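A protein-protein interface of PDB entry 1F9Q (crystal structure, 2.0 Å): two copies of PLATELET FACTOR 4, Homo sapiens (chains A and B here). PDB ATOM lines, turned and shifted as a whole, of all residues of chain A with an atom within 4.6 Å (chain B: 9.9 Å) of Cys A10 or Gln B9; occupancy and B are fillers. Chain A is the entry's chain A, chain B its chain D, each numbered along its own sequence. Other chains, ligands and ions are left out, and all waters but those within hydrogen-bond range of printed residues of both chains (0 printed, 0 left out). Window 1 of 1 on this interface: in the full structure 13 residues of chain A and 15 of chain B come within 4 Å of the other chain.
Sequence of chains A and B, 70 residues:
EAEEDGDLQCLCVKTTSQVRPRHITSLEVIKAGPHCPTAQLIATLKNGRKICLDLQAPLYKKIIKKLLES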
ATOM      1  N   GLN A   9      15.215 -15.953 -18.981  1.00  0.00           N
ATOM      2  CA  GLN A   9      15.171 -16.975 -20.019  1.00  0.00           C
ATOM      3  C   GLN A   9      15.289 -16.273 -21.377  1.00  0.00           C
ATOM      4  O   GLN A   9      15.387 -15.042 -21.432  1.00  0.00           O
ATOM      5  CB  GLN A   9      13.846 -17.753 -19.937  1.00  0.00           C
ATOM      6  CG  GLN A   9      12.587 -16.930 -20.258  1.00  0.00           C
ATOM      7  CD  GLN A   9      11.282 -17.698 -19.989  1.00  0.00           C
ATOM      8  OE1 GLN A   9      11.269 -18.928 -19.916  1.00  0.00           O
ATOM      9  NE2 GLN A   9      10.179 -16.966 -19.859  1.00  0.00           N
ATOM     10  N   CYS A  10      15.279 -17.042 -22.466  1.00  0.00           N
ATOM     11  CA  CYS A  10      15.354 -16.453 -23.805  1.00  0.00           C
ATOM     12  C   CYS A  10      14.111 -15.607 -24.044  1.00  0.00           C
ATOM     13  O   CYS A  10      12.992 -15.965 -23.635  1.00  0.00           O
ATOM     14  CB  CYS A  10      15.407 -17.519 -24.914  1.00  0.00           C
ATOM     15  SG  CYS A  10      16.799 -18.697 -24.867  1.00  0.00           S
ATOM     16  N   LEU A  11      14.311 -14.483 -24.710  1.00  0.00           N
ATOM     17  CA  LEU A  11      13.213 -13.611 -25.034  1.00  0.00           C
ATOM     18  C   LEU A  11      12.489 -14.232 -26.207  1.00  0.00           C
ATOM     19  O   LEU A  11      11.256 -14.269 -26.256  1.00  0.00           O
ATOM     20  CB  LEU A  11      13.751 -12.238 -25.415  1.00  0.00           C
ATOM     21  CG  LEU A  11      14.064 -11.380 -24.197  1.00  0.00           C
ATOM     22  CD1 LEU A  11      14.723 -10.086 -24.630  1.00  0.00           C
ATOM     23  CD2 LEU A  11      12.756 -11.097 -23.441  1.00  0.00           C
ATOM     24  N   CYS A  12      13.277 -14.749 -27.141  1.00  0.00           N
ATOM     25  CA  CYS A  12      12.751 -15.349 -28.361  1.00  0.00           C
ATOM     26  C   CYS A  12      12.352 -16.813 -28.244  1.00  0.00           C
ATOM     27  O   CYS A  12      13.143 -17.636 -27.782  1.00  0.00           O
ATOM     28  CB  CYS A  12      13.782 -15.214 -29.477  1.00  0.00           C
ATOM     29  SG  CYS A  12      14.275 -13.499 -29.853  1.00  0.00           S
ATOM     30  N   VAL A  13      11.124 -17.123 -28.663  1.00  0.00           N
ATOM     31  CA  VAL A  13      10.633 -18.503 -28.654  1.00  0.00           C
ATOM     32  C   VAL A  13      10.571 -18.972 -30.100  1.00  0.00           C
ATOM     33  O   VAL A  13      10.449 -20.156 -30.376  1.00  0.00           O
ATOM     34  CB  VAL A  13       9.223 -18.647 -28.026  1.00  0.00           C
ATOM     35  CG1 VAL A  13       9.255 -18.180 -26.595  1.00  0.00           C
ATOM     36  CG2 VAL A  13       8.195 -17.866 -28.832  1.00  0.00           C
ATOM     37  N   HIS A  35      21.007 -16.465 -19.478  1.00  0.00           N
ATOM     38  CA  HIS A  35      19.624 -16.167 -19.837  1.00  0.00           C
ATOM     39  C   HIS A  35      19.142 -16.951 -21.060  1.00  0.00           C
ATOM     40  O   HIS A  35      17.972 -17.334 -21.162  1.00  0.00           O
ATOM     41  CB  HIS A  35      19.520 -14.671 -20.124  1.00  0.00           C
ATOM     42  CG  HIS A  35      20.503 -14.205 -21.154  1.00  0.00           C
ATOM     43  ND1 HIS A  35      20.144 -13.947 -22.459  1.00  0.00           N
ATOM     44  CD2 HIS A  35      21.852 -14.089 -21.103  1.00  0.00           C
ATOM     45  CE1 HIS A  35      21.230 -13.700 -23.169  1.00  0.00           C
ATOM     46  NE2 HIS A  35      22.279 -13.781 -22.370  1.00  0.00           N
ATOM     47  N   CYS A  36      20.055 -17.158 -21.997  1.00  0.00           N
ATOM     48  CA  CYS A  36      19.751 -17.854 -23.227  1.00  0.00           C
ATOM     49  C   CYS A  36      21.072 -18.382 -23.752  1.00  0.00           C
ATOM     50  O   CYS A  36      22.031 -17.630 -23.900  1.00  0.00           O
ATOM     51  CB  CYS A  36      19.126 -16.892 -24.233  1.00  0.00           C
ATOM     52  SG  CYS A  36      18.369 -17.679 -25.684  1.00  0.00           S
ATOM     53  N   PRO A  37      21.138 -19.692 -24.020  1.00  0.00           N
ATOM     54  CA  PRO A  37      22.339 -20.361 -24.527  1.00  0.00           C
ATOM     55  C   PRO A  37      22.686 -19.972 -25.968  1.00  0.00           C
ATOM     56  O   PRO A  37      23.738 -20.342 -26.480  1.00  0.00           O
ATOM     57  CB  PRO A  37      21.980 -21.840 -24.387  1.00  0.00           C
ATOM     58  CG  PRO A  37      20.516 -21.849 -24.722  1.00  0.00           C
ATOM     59  CD  PRO A  37      20.004 -20.640 -23.938  1.00  0.00           C
ATOM     60  N   GLN A  40      20.545 -13.781 -29.841  1.00  0.00           N
ATOM     61  CA  GLN A  40      19.207 -13.459 -30.327  1.00  0.00           C
ATOM     62  C   GLN A  40      19.227 -12.117 -31.059  1.00  0.00           C
ATOM     63  O   GLN A  40      19.991 -11.221 -30.710  1.00  0.00           O
ATOM     64  CB  GLN A  40      18.223 -13.383 -29.161  1.00  0.00           C
ATOM     65  CG  GLN A  40      18.442 -14.424 -28.077  1.00  0.00           C
ATOM     66  CD  GLN A  40      17.457 -14.275 -26.931  1.00  0.00           C
ATOM     67  OE1 GLN A  40      16.262 -14.545 -27.089  1.00  0.00           O
ATOM     68  NE2 GLN A  40      17.950 -13.834 -25.773  1.00  0.00           N
ATOM     69  N   ASP B   5       0.078 -15.503 -31.644  1.00  0.00           N
ATOM     70  CA  ASP B   5       1.241 -15.570 -30.717  1.00  0.00           C
ATOM     71  C   ASP B   5       2.503 -15.023 -31.363  1.00  0.00           C
ATOM     72  O   ASP B   5       2.888 -15.440 -32.458  1.00  0.00           O
ATOM     73  CB  ASP B   5       1.479 -17.009 -30.255  1.00  0.00           C
ATOM     74  CG  ASP B   5       0.649 -17.377 -29.034  1.00  0.00           C
ATOM     75  OD1 ASP B   5       0.826 -18.499 -28.508  1.00  0.00           O
ATOM     76  OD2 ASP B   5      -0.176 -16.543 -28.597  1.00  0.00           O
ATOM     77  N   GLY B   6       3.145 -14.089 -30.666  1.00  0.00           N
ATOM     78  CA  GLY B   6       4.352 -13.472 -31.179  1.00  0.00           C
ATOM     79  C   GLY B   6       5.629 -14.247 -30.937  1.00  0.00           C
ATOM     80  O   GLY B   6       5.622 -15.357 -30.390  1.00  0.00           O
ATOM     81  N   ASP B   7       6.736 -13.639 -31.345  1.00  0.00           N
ATOM     82  CA  ASP B   7       8.058 -14.226 -31.215  1.00  0.00           C
ATOM     83  C   ASP B   7       8.628 -14.124 -29.810  1.00  0.00           C
ATOM     84  O   ASP B   7       9.509 -14.894 -29.447  1.00  0.00           O
ATOM     85  CB  ASP B   7       9.033 -13.533 -32.168  1.00  0.00           C
ATOM     86  CG  ASP B   7       8.687 -13.742 -33.623  1.00  0.00           C
ATOM     87  OD1 ASP B   7       9.481 -13.271 -34.464  1.00  0.00           O
ATOM     88  OD2 ASP B   7       7.642 -14.368 -33.926  1.00  0.00           O
ATOM     89  N   LEU B   8       8.122 -13.176 -29.029  1.00  0.00           N
ATOM     90  CA  LEU B   8       8.638 -12.960 -27.687  1.00  0.00           C
ATOM     91  C   LEU B   8       7.807 -13.455 -26.515  1.00  0.00           C
ATOM     92  O   LEU B   8       6.571 -13.529 -26.573  1.00  0.00           O
ATOM     93  CB  LEU B   8       8.918 -11.464 -27.480  1.00  0.00           C
ATOM     94  CG  LEU B   8      10.134 -10.801 -28.147  1.00  0.00           C
ATOM     95  CD1 LEU B   8       9.969 -10.801 -29.650  1.00  0.00           C
ATOM     96  CD2 LEU B   8      10.284  -9.364 -27.638  1.00  0.00           C
ATOM     97  N   GLN B   9       8.514 -13.793 -25.440  1.00  0.00           N
ATOM     98  CA  GLN B   9       7.881 -14.218 -24.204  1.00  0.00           C
ATOM     99  C   GLN B   9       8.513 -13.382 -23.110  1.00  0.00           C
ATOM    100  O   GLN B   9       9.432 -12.608 -23.373  1.00  0.00           O
ATOM    101  CB  GLN B   9       8.130 -15.697 -23.922  1.00  0.00           C
ATOM    102  CG  GLN B   9       9.573 -16.062 -23.671  1.00  0.00           C
ATOM    103  CD  GLN B   9       9.746 -17.558 -23.463  1.00  0.00           C
ATOM    104  OE1 GLN B   9      10.862 -18.060 -23.328  1.00  0.00           O
ATOM    105  NE2 GLN B   9       8.628 -18.279 -23.438  1.00  0.00           N
ATOM    106  N   CYS B  10       8.017 -13.525 -21.887  1.00  0.00           N
ATOM    107  CA  CYS B  10       8.567 -12.785 -20.764  1.00  0.00           C
ATOM    108  C   CYS B  10      10.018 -13.222 -20.547  1.00  0.00           C
ATOM    109  O   CYS B  10      10.352 -14.405 -20.655  1.00  0.00           O
ATOM    110  CB  CYS B  10       7.763 -13.059 -19.486  1.00  0.00           C
ATOM    111  SG  CYS B  10       5.970 -12.696 -19.547  1.00  0.00           S
ATOM    112  N   LEU B  11      10.873 -12.253 -20.244  1.00  0.00           N
ATOM    113  CA  LEU B  11      12.288 -12.507 -19.996  1.00  0.00           C
ATOM    114  C   LEU B  11      12.432 -13.113 -18.594  1.00  0.00           C
ATOM    115  O   LEU B  11      13.322 -13.928 -18.324  1.00  0.00           O
ATOM    116  CB  LEU B  11      13.049 -11.180 -20.107  1.00  0.00           C
ATOM    117  CG  LEU B  11      14.569 -11.156 -20.027  1.00  0.00           C
ATOM    118  CD1 LEU B  11      15.174 -12.058 -21.091  1.00  0.00           C
ATOM    119  CD2 LEU B  11      15.030  -9.720 -20.216  1.00  0.00           C
ATOM    120  N   CYS B  12      11.527 -12.717 -17.713  1.00  0.00           N
ATOM    121  CA  CYS B  12      11.508 -13.195 -16.342  1.00  0.00           C
ATOM    122  C   CYS B  12      10.722 -14.496 -16.200  1.00  0.00           C
ATOM    123  O   CYS B  12       9.502 -14.521 -16.364  1.00  0.00           O
ATOM    124  CB  CYS B  12      10.898 -12.130 -15.432  1.00  0.00           C
ATOM    125  SG  CYS B  12      11.910 -10.621 -15.301  1.00  0.00           S
ATOM    126  N   VAL B  13      11.433 -15.572 -15.886  1.00  0.00           N
ATOM    127  CA  VAL B  13      10.812 -16.872 -15.718  1.00  0.00           C
ATOM    128  C   VAL B  13      10.511 -17.097 -14.239  1.00  0.00           C
ATOM    129  O   VAL B  13       9.697 -17.941 -13.883  1.00  0.00           O
ATOM    130  CB  VAL B  13      11.733 -17.998 -16.276  1.00  0.00           C
ATOM    131  CG1 VAL B  13      12.825 -18.329 -15.275  1.00  0.00           C
ATOM    132  CG2 VAL B  13      10.895 -19.227 -16.655  1.00  0.00           C
ATOM    133  N   ILE B  30       9.900  -2.879 -17.362  1.00  0.00           N
ATOM    134  CA  ILE B  30       9.284  -3.189 -18.635  1.00  0.00           C
ATOM    135  C   ILE B  30       7.775  -3.353 -18.452  1.00  0.00           C
ATOM    136  O   ILE B  30       7.311  -4.165 -17.651  1.00  0.00           O
ATOM    137  CB  ILE B  30       9.921  -4.466 -19.244  1.00  0.00           C
ATOM    138  CG1 ILE B  30      11.447  -4.316 -19.234  1.00  0.00           C
ATOM    139  CG2 ILE B  30       9.416  -4.690 -20.682  1.00  0.00           C
ATOM    140  CD1 ILE B  30      12.215  -5.542 -19.688  1.00  0.00           C
ATOM    141  N   LYS B  31       7.030  -2.527 -19.185  1.00  0.00           N
ATOM    142  CA  LYS B  31       5.572  -2.520 -19.162  1.00  0.00           C
ATOM    143  C   LYS B  31       5.031  -3.723 -19.920  1.00  0.00           C
ATOM    144  O   LYS B  31       5.653  -4.218 -20.859  1.00  0.00           O
ATOM    145  CB  LYS B  31       5.055  -1.246 -19.820  1.00  0.00           C
ATOM    146  CG  LYS B  31       3.550  -1.131 -19.928  1.00  0.00           C
ATOM    147  CD  LYS B  31       3.165   0.142 -20.677  1.00  0.00           C
ATOM    148  CE  LYS B  31       1.654   0.379 -20.645  1.00  0.00           C
ATOM    149  NZ  LYS B  31       1.270   1.709 -21.215  1.00  0.00           N
ATOM    150  N   GLY B  33       2.800  -6.020 -22.406  1.00  0.00           N
ATOM    151  CA  GLY B  33       2.473  -5.857 -23.805  1.00  0.00           C
ATOM    152  C   GLY B  33       2.393  -7.235 -24.420  1.00  0.00           C
ATOM    153  O   GLY B  33       2.344  -8.221 -23.689  1.00  0.00           O
ATOM    154  N   PRO B  34       2.390  -7.337 -25.758  1.00  0.00           N
ATOM    155  CA  PRO B  34       2.315  -8.596 -26.516  1.00  0.00           C
ATOM    156  C   PRO B  34       3.385  -9.601 -26.106  1.00  0.00           C
ATOM    157  O   PRO B  34       3.200 -10.811 -26.227  1.00  0.00           O
ATOM    158  CB  PRO B  34       2.517  -8.144 -27.962  1.00  0.00           C
ATOM    159  CG  PRO B  34       1.977  -6.731 -27.957  1.00  0.00           C
ATOM    160  CD  PRO B  34       2.534  -6.189 -26.668  1.00  0.00           C
ATOM    161  N   HIS B  35       4.502  -9.076 -25.629  1.00  0.00           N
ATOM    162  CA  HIS B  35       5.652  -9.868 -25.223  1.00  0.00           C
ATOM    163  C   HIS B  35       5.519 -10.492 -23.848  1.00  0.00           C
ATOM    164  O   HIS B  35       6.166 -11.494 -23.555  1.00  0.00           O
ATOM    165  CB  HIS B  35       6.890  -8.980 -25.212  1.00  0.00           C
ATOM    166  CG  HIS B  35       6.806  -7.866 -24.216  1.00  0.00           C
ATOM    167  ND1 HIS B  35       5.991  -6.765 -24.399  1.00  0.00           N
ATOM    168  CD2 HIS B  35       7.354  -7.726 -22.985  1.00  0.00           C
ATOM    169  CE1 HIS B  35       6.039  -6.002 -23.321  1.00  0.00           C
ATOM    170  NE2 HIS B  35       6.858  -6.564 -22.450  1.00  0.00           N
ATOM    171  N   CYS B  36       4.695  -9.886 -22.997  1.00  0.00           N
ATOM    172  CA  CYS B  36       4.536 -10.367 -21.629  1.00  0.00           C
ATOM    173  C   CYS B  36       3.273  -9.775 -20.993  1.00  0.00           C
ATOM    174  O   CYS B  36       3.078  -8.563 -21.010  1.00  0.00           O
ATOM    175  CB  CYS B  36       5.783  -9.973 -20.817  1.00  0.00           C
ATOM    176  SG  CYS B  36       5.861 -10.704 -19.157  1.00  0.00           S
ATOM    177  N   PRO B  37       2.403 -10.629 -20.423  1.00  0.00           N
ATOM    178  CA  PRO B  37       1.149 -10.194 -19.783  1.00  0.00           C
ATOM    179  C   PRO B  37       1.348  -9.361 -18.511  1.00  0.00           C
ATOM    180  O   PRO B  37       0.457  -8.633 -18.081  1.00  0.00           O
ATOM    181  CB  PRO B  37       0.428 -11.515 -19.472  1.00  0.00           C
ATOM    182  CG  PRO B  37       1.064 -12.522 -20.412  1.00  0.00           C
ATOM    183  CD  PRO B  37       2.511 -12.098 -20.433  1.00  0.00           C
ATOM    184  N   THR B  38       2.530  -9.464 -17.925  1.00  0.00           N
ATOM    185  CA  THR B  38       2.829  -8.770 -16.683  1.00  0.00           C
ATOM    186  C   THR B  38       3.976  -7.775 -16.835  1.00  0.00           C
ATOM    187  O   THR B  38       4.727  -7.818 -17.813  1.00  0.00           O
ATOM    188  CB  THR B  38       3.222  -9.803 -15.606  1.00  0.00           C
ATOM    189  OG1 THR B  38       3.363  -9.163 -14.333  1.00  0.00           O
ATOM    190  CG2 THR B  38       4.540 -10.457 -15.981  1.00  0.00           C
ATOM    191  N   GLN B  40       7.612  -6.171 -15.634  1.00  0.00           N
ATOM    192  CA  GLN B  40       8.823  -6.858 -15.204  1.00  0.00           C
ATOM    193  C   GLN B  40       9.829  -5.854 -14.657  1.00  0.00           C
ATOM    194  O   GLN B  40       9.964  -4.746 -15.175  1.00  0.00           O
ATOM    195  CB  GLN B  40       9.452  -7.633 -16.362  1.00  0.00           C
ATOM    196  CG  GLN B  40       8.565  -8.703 -16.965  1.00  0.00           C
ATOM    197  CD  GLN B  40       9.119  -9.206 -18.278  1.00  0.00           C
ATOM    198  OE1 GLN B  40       9.868 -10.183 -18.328  1.00  0.00           O
ATOM    199  NE2 GLN B  40       8.768  -8.518 -19.360  1.00  0.00           N
ATOM    200  N   ILE B  42      13.683  -5.853 -13.962  1.00  0.00           N
ATOM    201  CA  ILE B  42      14.956  -6.527 -14.132  1.00  0.00           C
ATOM    202  C   ILE B  42      16.084  -5.694 -13.533  1.00  0.00           C
ATOM    203  O   ILE B  42      16.340  -4.560 -13.942  1.00  0.00           O
ATOM    204  CB  ILE B  42      15.207  -6.826 -15.630  1.00  0.00           C
ATOM    205  CG1 ILE B  42      14.042  -7.672 -16.163  1.00  0.00           C
ATOM    206  CG2 ILE B  42      16.531  -7.576 -15.820  1.00  0.00           C
ATOM    207  CD1 ILE B  42      14.132  -7.988 -17.630  1.00  0.00           C
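Gln A9 touches its own counterpart, Gln B9. Gln A9 touches Cys B10, and with the chains exchanged Cys A10 touches Gln B9. Gln A9 touches Leu B11, and with the chains exchanged Leu A11 touches Gln B9. Gln A9 touches Val B13, and with the chains exchanged Val A13 touches Gln B9. Of the 13 pairs that touch across the chains among the printed residues, 8 have their exchanged pair printed and touching as well.
Gln A9 touches Gln B9 (CD to OE1, 3.4 Å). Gln A9 touches Val B13. O of Leu A11 touches O of Asp B7, 3.7 Å away. Leu A11 touches Leu B8. Leu A11 touches Leu B11. CA of Cys A12 touches O of Asp B7, at 3.4 Å. Val A13 touches Gly B6 (CG2 to O, 3.9 Å). Gln B9 touches Val A13.
Hydrophobic or aromatic side chains of chain B within 4 Å of the printed part of chain A: Leu B8, Leu B11 and Val B13. Among the printed residues, 13 pairs touch across the chains.
Gln A9 touches four residues of chain B. Cys A10 touches just one residue of chain B: Gln B9. His A35 touches none of the printed residues of chain B. No residue of chain B comes within 4 Å of Cys A36. Of the printed residues of chain A, Gln B9 touches Gln A9 (3.4 Å), Cys A10 (3.0 Å), Leu A11 (2.9 Å) and Val A13 (3.2 Å). Printed residues of chain A within 4 Å of Cys B10: Gln A9. Of the printed residues of chain A, Leu B11 touches Gln A9 and Leu A11. Of the printed residues of chain A, Val B13 touches Gln A9 (3.3 Å). Gln B40 touches none of the printed residues of chain A. The nearest printed residue of chain A that does not touch Gln B9 is Cys A12 (5.0 Å). The nearest printed residue of chain A that does not touch Val B13 is Cys A10 (7.2 Å).
The side-chain amide oxygen (OE1) of Gln A40 is in hydrogen-bond range of the backbone NH (N) of Cys A12 (3.0 Å). The side-chain sulfur (SG) of Cys A36 is disulfide-bonded to the side-chain sulfur (SG) of Cys A10 (2.0 Å). O of His A35 lies within hydrogen-bond range of N of Cys A10, at 3.0 Å. The backbone NH (N) of Cys B10 sits at hydrogen-bond distance from the backbone carbonyl oxygen (O) of His B35, 3.2 Å away. The side-chain amide oxygen (OE1) of Gln A40 lies within hydrogen-bond range of the backbone NH (N) of Leu A11, at 3.1 Å. The backbone NH of Leu B11 is in hydrogen-bond range of the side-chain amide oxygen of Gln B40, at 3.0 Å.
N of Gln A9 sits at hydrogen-bond distance from O of Leu B11, at 2.8 Å. The backbone carbonyl oxygen (O) of Cys B10 lies within hydrogen-bond range of the side-chain amide nitrogen (NE2) of Gln A9 (2.7 Å). O of Asp B7 is in hydrogen-bond range of N of Val A13 (2.9 Å). O of Leu A11 sits at hydrogen-bond distance from N of Gln B9 (2.9 Å). The side-chain amide oxygen (OE1) of Gln B9 lies close to the backbone carbonyl oxygen (O) of Cys A10, at 3.0 Å.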
